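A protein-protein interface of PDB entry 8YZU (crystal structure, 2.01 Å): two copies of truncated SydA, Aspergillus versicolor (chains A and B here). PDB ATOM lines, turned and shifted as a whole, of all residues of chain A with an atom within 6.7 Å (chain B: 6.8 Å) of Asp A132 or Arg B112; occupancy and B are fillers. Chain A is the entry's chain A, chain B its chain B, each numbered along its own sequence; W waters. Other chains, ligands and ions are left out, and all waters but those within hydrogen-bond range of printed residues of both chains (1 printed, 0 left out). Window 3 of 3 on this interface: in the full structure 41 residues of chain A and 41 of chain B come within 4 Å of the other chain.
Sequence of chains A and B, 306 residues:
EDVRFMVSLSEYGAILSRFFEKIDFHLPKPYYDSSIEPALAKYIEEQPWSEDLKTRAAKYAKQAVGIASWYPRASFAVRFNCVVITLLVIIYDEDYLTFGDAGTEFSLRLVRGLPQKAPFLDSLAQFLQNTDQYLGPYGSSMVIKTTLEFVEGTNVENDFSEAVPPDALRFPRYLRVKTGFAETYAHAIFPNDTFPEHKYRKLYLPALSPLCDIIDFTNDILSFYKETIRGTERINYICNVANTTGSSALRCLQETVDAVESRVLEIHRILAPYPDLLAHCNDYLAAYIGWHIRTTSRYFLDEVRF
The guanidinium group (NH2) of Arg B112 lies within salt-bridge range of the side-chain carboxylate (OD1) of Asp A132 (2.7 Å).
The backbone carbonyl oxygen (O) of Val B111 is in hydrogen-bond range of the side-chain amide nitrogen (NE2) of Gln A129, 2.9 Å away.
O of Gln A129 sits at hydrogen-bond distance from NH2 of Arg B112, at 2.7 Å.
Of the printed residues of chain B, Leu A110 touches Leu B110 (3.9 Å) and Val B111 (3.8 Å).
Printed residues of chain B within 4 Å of Gln A129: Leu B108 (3.8 Å), Val B111 (2.9 Å) and Arg B112 (2.7 Å).
Asn A130 touches none of the printed residues of chain B.
Of chain B, only Leu B108 and Arg B112 come within 4 Å of Asp A132.
Ser B107 touches none of the printed residues of chain A.
Arg B112 touches two residues of chain A.
Of the 8 printed residues of chain B, 4 touch a printed residue of chain A.
Hydrophobic or aromatic side chains of chain A that line the printed part of chain B: Leu A110.
Along chain A the printed residues that touch a printed residue of chain B span positions 110 to 132.
Among the printed residues, 8 pairs touch across the chains.
Among the printed residues, Asp or Glu carboxylates within 4 Å of a Lys or Arg side-chain nitrogen of the other chain: Asp A132 with Arg B112.
Among the printed residues, pairs that only touch across the chains: Leu A110 with Leu B110, Leu A110 with Val B111, Leu A128 with Leu B108, Gln A129 with Leu B108 and Asp A132 with Leu B108.
Leu B110 touches its own counterpart, Leu A110.
Of the 8 pairs that touch across the chains among the printed residues, 1 has its exchanged pair printed and touching as well.
Water W1 lies within hydrogen-bond range of the backbone carbonyl oxygen of Val B111, the backbone carbonyl oxygen of Leu A110 and the side-chain amide nitrogen of Gln A129.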
ATOM      1  N   LEU A 110      -6.037  13.903  32.944  1.00  0.00           N
ATOM      2  CA  LEU A 110      -7.037  14.565  32.109  1.00  0.00           C
ATOM      3  C   LEU A 110      -8.457  14.181  32.534  1.00  0.00           C
ATOM      4  O   LEU A 110      -9.291  15.053  32.801  1.00  0.00           O
ATOM      5  CB  LEU A 110      -6.808  14.214  30.633  1.00  0.00           C
ATOM      6  CG  LEU A 110      -7.720  14.877  29.597  1.00  0.00           C
ATOM      7  CD1 LEU A 110      -7.534  16.381  29.641  1.00  0.00           C
ATOM      8  CD2 LEU A 110      -7.430  14.391  28.196  1.00  0.00           C
ATOM      9  N   GLY A 113      -9.792  15.450  35.721  1.00  0.00           N
ATOM     10  CA  GLY A 113      -9.839  16.896  35.873  1.00  0.00           C
ATOM     11  C   GLY A 113      -8.751  17.440  36.779  1.00  0.00           C
ATOM     12  O   GLY A 113      -9.004  18.363  37.563  1.00  0.00           O
ATOM     13  N   PHE A 127      -6.303  22.652  24.951  1.00  0.00           N
ATOM     14  CA  PHE A 127      -6.692  22.594  23.544  1.00  0.00           C
ATOM     15  C   PHE A 127      -7.814  21.586  23.338  1.00  0.00           C
ATOM     16  O   PHE A 127      -8.801  21.876  22.650  1.00  0.00           O
ATOM     17  CB  PHE A 127      -5.492  22.246  22.641  1.00  0.00           C
ATOM     18  CG  PHE A 127      -5.861  22.134  21.182  1.00  0.00           C
ATOM     19  CD1 PHE A 127      -6.337  20.936  20.657  1.00  0.00           C
ATOM     20  CD2 PHE A 127      -5.817  23.237  20.355  1.00  0.00           C
ATOM     21  CE1 PHE A 127      -6.742  20.831  19.315  1.00  0.00           C
ATOM     22  CE2 PHE A 127      -6.201  23.136  19.008  1.00  0.00           C
ATOM     23  CZ  PHE A 127      -6.665  21.927  18.493  1.00  0.00           C
ATOM     24  N   LEU A 128      -7.674  20.393  23.938  1.00  0.00           N
ATOM     25  CA  LEU A 128      -8.668  19.331  23.816  1.00  0.00           C
ATOM     26  C   LEU A 128     -10.029  19.759  24.337  1.00  0.00           C
ATOM     27  O   LEU A 128     -11.059  19.234  23.886  1.00  0.00           O
ATOM     28  CB  LEU A 128      -8.213  18.093  24.587  1.00  0.00           C
ATOM     29  CG  LEU A 128      -6.966  17.362  24.093  1.00  0.00           C
ATOM     30  CD1 LEU A 128      -6.739  16.111  24.932  1.00  0.00           C
ATOM     31  CD2 LEU A 128      -7.106  17.003  22.618  1.00  0.00           C
ATOM     32  N   GLN A 129     -10.047  20.668  25.317  1.00  0.00           N
ATOM     33  CA  GLN A 129     -11.272  21.147  25.930  1.00  0.00           C
ATOM     34  C   GLN A 129     -12.000  22.161  25.062  1.00  0.00           C
ATOM     35  O   GLN A 129     -13.165  22.458  25.332  1.00  0.00           O
ATOM     36  CB  GLN A 129     -10.964  21.775  27.310  1.00  0.00           C
ATOM     37  CG  GLN A 129     -10.399  20.793  28.346  1.00  0.00           C
ATOM     38  CD  GLN A 129      -9.790  21.488  29.564  1.00  0.00           C
ATOM     39  OE1 GLN A 129      -9.615  22.702  29.576  1.00  0.00           O
ATOM     40  NE2 GLN A 129      -9.459  20.708  30.589  1.00  0.00           N
ATOM     41  N   ASN A 130     -11.358  22.707  24.031  1.00  0.00           N
ATOM     42  CA  ASN A 130     -11.986  23.777  23.266  1.00  0.00           C
ATOM     43  C   ASN A 130     -12.159  23.445  21.790  1.00  0.00           C
ATOM     44  O   ASN A 130     -12.366  24.357  20.980  1.00  0.00           O
ATOM     45  CB  ASN A 130     -11.209  25.087  23.423  1.00  0.00           C
ATOM     46  CG  ASN A 130     -11.338  25.662  24.814  1.00  0.00           C
ATOM     47  OD1 ASN A 130     -10.658  25.237  25.747  1.00  0.00           O
ATOM     48  ND2 ASN A 130     -12.303  26.543  24.984  1.00  0.00           N
ATOM     49  N   THR A 131     -12.124  22.165  21.417  1.00  0.00           N
ATOM     50  CA  THR A 131     -12.280  21.842  20.005  1.00  0.00           C
ATOM     51  C   THR A 131     -13.681  22.123  19.480  1.00  0.00           C
ATOM     52  O   THR A 131     -13.857  22.167  18.253  1.00  0.00           O
ATOM     53  CB  THR A 131     -11.914  20.382  19.739  1.00  0.00           C
ATOM     54  OG1 THR A 131     -12.575  19.543  20.693  1.00  0.00           O
ATOM     55  CG2 THR A 131     -10.412  20.194  19.846  1.00  0.00           C
ATOM     56  N   ASP A 132     -14.669  22.344  20.361  1.00  0.00           N
ATOM     57  CA  ASP A 132     -15.999  22.700  19.888  1.00  0.00           C
ATOM     58  C   ASP A 132     -16.005  24.050  19.190  1.00  0.00           C
ATOM     59  O   ASP A 132     -16.959  24.356  18.473  1.00  0.00           O
ATOM     60  CB  ASP A 132     -17.007  22.702  21.045  1.00  0.00           C
ATOM     61  CG  ASP A 132     -16.528  23.519  22.255  1.00  0.00           C
ATOM     62  OD1 ASP A 132     -17.318  23.685  23.210  1.00  0.00           O
ATOM     63  OD2 ASP A 132     -15.383  24.004  22.249  1.00  0.00           O
ATOM     64  N   GLN A 133     -14.956  24.860  19.366  1.00  0.00           N
ATOM     65  CA  GLN A 133     -14.841  26.090  18.590  1.00  0.00           C
ATOM     66  C   GLN A 133     -14.794  25.832  17.087  1.00  0.00           C
ATOM     67  O   GLN A 133     -15.126  26.739  16.315  1.00  0.00           O
ATOM     68  CB  GLN A 133     -13.596  26.891  19.001  1.00  0.00           C
ATOM     69  CG  GLN A 133     -13.653  27.464  20.396  1.00  0.00           C
ATOM     70  CD  GLN A 133     -14.849  28.375  20.606  1.00  0.00           C
ATOM     71  OE1 GLN A 133     -15.261  29.115  19.703  1.00  0.00           O
ATOM     72  NE2 GLN A 133     -15.442  28.301  21.797  1.00  0.00           N
ATOM     73  N   TYR A 134     -14.378  24.632  16.641  1.00  0.00           N
ATOM     74  CA  TYR A 134     -14.353  24.362  15.209  1.00  0.00           C
ATOM     75  C   TYR A 134     -14.828  22.972  14.798  1.00  0.00           C
ATOM     76  O   TYR A 134     -14.970  22.727  13.592  1.00  0.00           O
ATOM     77  CB  TYR A 134     -12.936  24.618  14.635  1.00  0.00           C
ATOM     78  CG  TYR A 134     -11.862  23.643  15.057  1.00  0.00           C
ATOM     79  CD1 TYR A 134     -11.308  23.690  16.335  1.00  0.00           C
ATOM     80  CD2 TYR A 134     -11.373  22.691  14.162  1.00  0.00           C
ATOM     81  CE1 TYR A 134     -10.320  22.790  16.723  1.00  0.00           C
ATOM     82  CE2 TYR A 134     -10.379  21.788  14.536  1.00  0.00           C
ATOM     83  CZ  TYR A 134      -9.858  21.835  15.816  1.00  0.00           C
ATOM     84  OH  TYR A 134      -8.864  20.933  16.162  1.00  0.00           O
ATOM     85  N   LEU A 135     -15.145  22.079  15.739  1.00  0.00           N
ATOM     86  CA  LEU A 135     -15.591  20.734  15.408  1.00  0.00           C
ATOM     87  C   LEU A 135     -16.893  20.405  16.133  1.00  0.00           C
ATOM     88  O   LEU A 135     -17.208  20.969  17.193  1.00  0.00           O
ATOM     89  CB  LEU A 135     -14.541  19.684  15.773  1.00  0.00           C
ATOM     90  CG  LEU A 135     -13.189  19.787  15.074  1.00  0.00           C
ATOM     91  CD1 LEU A 135     -12.220  18.848  15.732  1.00  0.00           C
ATOM     92  CD2 LEU A 135     -13.311  19.475  13.586  1.00  0.00           C
ATOM     93  N   GLY A 136     -17.647  19.467  15.538  1.00  0.00           N
ATOM     94  CA  GLY A 136     -18.799  18.889  16.184  1.00  0.00           C
ATOM     95  C   GLY A 136     -18.389  17.849  17.202  1.00  0.00           C
ATOM     96  O   GLY A 136     -17.207  17.589  17.425  1.00  0.00           O
ATOM     97  N   SER A 140     -14.766  16.322  17.954  1.00  0.00           N
ATOM     98  CA  SER A 140     -14.130  16.648  19.229  1.00  0.00           C
ATOM     99  C   SER A 140     -13.688  15.393  19.969  1.00  0.00           C
ATOM    100  O   SER A 140     -12.625  15.389  20.599  1.00  0.00           O
ATOM    101  CB  SER A 140     -15.072  17.476  20.108  1.00  0.00           C
ATOM    102  OG  SER A 140     -15.350  18.729  19.506  1.00  0.00           O
ATOM    103  N   ASN A 192     -16.909  21.925  11.184  1.00  0.00           N
ATOM    104  CA  ASN A 192     -18.309  21.901  11.586  1.00  0.00           C
ATOM    105  C   ASN A 192     -19.068  23.158  11.147  1.00  0.00           C
ATOM    106  O   ASN A 192     -20.284  23.098  10.948  1.00  0.00           O
ATOM    107  CB  ASN A 192     -18.394  21.713  13.107  1.00  0.00           C
ATOM    108  CG  ASN A 192     -19.770  21.260  13.584  1.00  0.00           C
ATOM    109  OD1 ASN A 192     -20.326  20.272  13.090  1.00  0.00           O
ATOM    110  ND2 ASN A 192     -20.328  21.988  14.551  1.00  0.00           N
ATOM    111  N   SER B 107     -17.598  13.253  25.834  1.00  0.00           N
ATOM    112  CA  SER B 107     -16.141  13.376  25.738  1.00  0.00           C
ATOM    113  C   SER B 107     -15.660  14.750  26.207  1.00  0.00           C
ATOM    114  O   SER B 107     -14.664  14.844  26.930  1.00  0.00           O
ATOM    115  CB  SER B 107     -15.661  13.072  24.314  1.00  0.00           C
ATOM    116  OG  SER B 107     -16.116  14.046  23.391  1.00  0.00           O
ATOM    117  N   LEU B 108     -16.357  15.826  25.825  1.00  0.00           N
ATOM    118  CA  LEU B 108     -15.927  17.162  26.236  1.00  0.00           C
ATOM    119  C   LEU B 108     -16.109  17.371  27.735  1.00  0.00           C
ATOM    120  O   LEU B 108     -15.251  17.966  28.388  1.00  0.00           O
ATOM    121  CB  LEU B 108     -16.679  18.237  25.445  1.00  0.00           C
ATOM    122  CG  LEU B 108     -16.073  18.627  24.084  1.00  0.00           C
ATOM    123  CD1 LEU B 108     -16.976  19.613  23.368  1.00  0.00           C
ATOM    124  CD2 LEU B 108     -14.656  19.191  24.215  1.00  0.00           C
ATOM    125  N   ARG B 109     -17.226  16.911  28.303  1.00  0.00           N
ATOM    126  CA  ARG B 109     -17.398  17.047  29.748  1.00  0.00           C
ATOM    127  C   ARG B 109     -16.341  16.242  30.492  1.00  0.00           C
ATOM    128  O   ARG B 109     -15.840  16.677  31.535  1.00  0.00           O
ATOM    129  CB  ARG B 109     -18.799  16.604  30.161  1.00  0.00           C
ATOM    130  CG  ARG B 109     -19.866  17.523  29.676  1.00  0.00           C
ATOM    131  CD  ARG B 109     -21.186  17.182  30.285  1.00  0.00           C
ATOM    132  NE  ARG B 109     -22.254  17.984  29.708  1.00  0.00           N
ATOM    133  CZ  ARG B 109     -23.133  18.630  30.463  1.00  0.00           C
ATOM    134  NH1 ARG B 109     -23.067  18.574  31.783  1.00  0.00           N
ATOM    135  NH2 ARG B 109     -24.077  19.375  29.883  1.00  0.00           N
ATOM    136  N   LEU B 110     -15.991  15.065  29.962  1.00  0.00           N
ATOM    137  CA  LEU B 110     -14.955  14.235  30.573  1.00  0.00           C
ATOM    138  C   LEU B 110     -13.620  14.980  30.656  1.00  0.00           C
ATOM    139  O   LEU B 110     -13.023  15.089  31.735  1.00  0.00           O
ATOM    140  CB  LEU B 110     -14.797  12.939  29.776  1.00  0.00           C
ATOM    141  CG  LEU B 110     -13.876  11.881  30.393  1.00  0.00           C
ATOM    142  CD1 LEU B 110     -14.504  11.344  31.667  1.00  0.00           C
ATOM    143  CD2 LEU B 110     -13.592  10.742  29.403  1.00  0.00           C
ATOM    144  N   VAL B 111     -13.144  15.522  29.528  1.00  0.00           N
ATOM    145  CA  VAL B 111     -11.838  16.179  29.547  1.00  0.00           C
ATOM    146  C   VAL B 111     -11.897  17.596  30.103  1.00  0.00           C
ATOM    147  O   VAL B 111     -10.847  18.178  30.389  1.00  0.00           O
ATOM    148  CB  VAL B 111     -11.187  16.186  28.152  1.00  0.00           C
ATOM    149  CG1 VAL B 111     -11.149  14.766  27.581  1.00  0.00           C
ATOM    150  CG2 VAL B 111     -11.892  17.155  27.222  1.00  0.00           C
ATOM    151  N   ARG B 112     -13.088  18.177  30.259  1.00  0.00           N
ATOM    152  CA  ARG B 112     -13.207  19.420  31.005  1.00  0.00           C
ATOM    153  C   ARG B 112     -13.310  19.189  32.503  1.00  0.00           C
ATOM    154  O   ARG B 112     -13.258  20.158  33.268  1.00  0.00           O
ATOM    155  CB  ARG B 112     -14.416  20.213  30.521  1.00  0.00           C
ATOM    156  CG  ARG B 112     -14.188  20.889  29.196  1.00  0.00           C
ATOM    157  CD  ARG B 112     -15.488  21.365  28.577  1.00  0.00           C
ATOM    158  NE  ARG B 112     -15.240  22.005  27.293  1.00  0.00           N
ATOM    159  CZ  ARG B 112     -16.173  22.460  26.469  1.00  0.00           C
ATOM    160  NH1 ARG B 112     -17.461  22.346  26.749  1.00  0.00           N
ATOM    161  NH2 ARG B 112     -15.804  23.042  25.332  1.00  0.00           N
ATOM    162  N   GLY B 113     -13.408  17.938  32.942  1.00  0.00           N
ATOM    163  CA  GLY B 113     -13.588  17.649  34.351  1.00  0.00           C
ATOM    164  C   GLY B 113     -14.963  17.986  34.878  1.00  0.00           C
ATOM    165  O   GLY B 113     -15.116  18.234  36.076  1.00  0.00           O
ATOM    166  N   LEU B 114     -15.988  18.001  34.005  1.00  0.00           N
ATOM    167  CA  LEU B 114     -17.330  18.392  34.414  1.00  0.00           C
ATOM    168  C   LEU B 114     -18.169  17.174  34.777  1.00  0.00           C
ATOM    169  O   LEU B 114     -17.952  16.078  34.242  1.00  0.00           O
ATOM    170  CB  LEU B 114     -18.046  19.162  33.297  1.00  0.00           C
ATOM    171  CG  LEU B 114     -17.266  20.294  32.646  1.00  0.00           C
ATOM    172  CD1 LEU B 114     -18.113  21.021  31.599  1.00  0.00           C
ATOM    173  CD2 LEU B 114     -16.765  21.242  33.716  1.00  0.00           C
HETATM  174  O   HOH W   1      -8.834  18.054  32.647  1.00  0.00           O
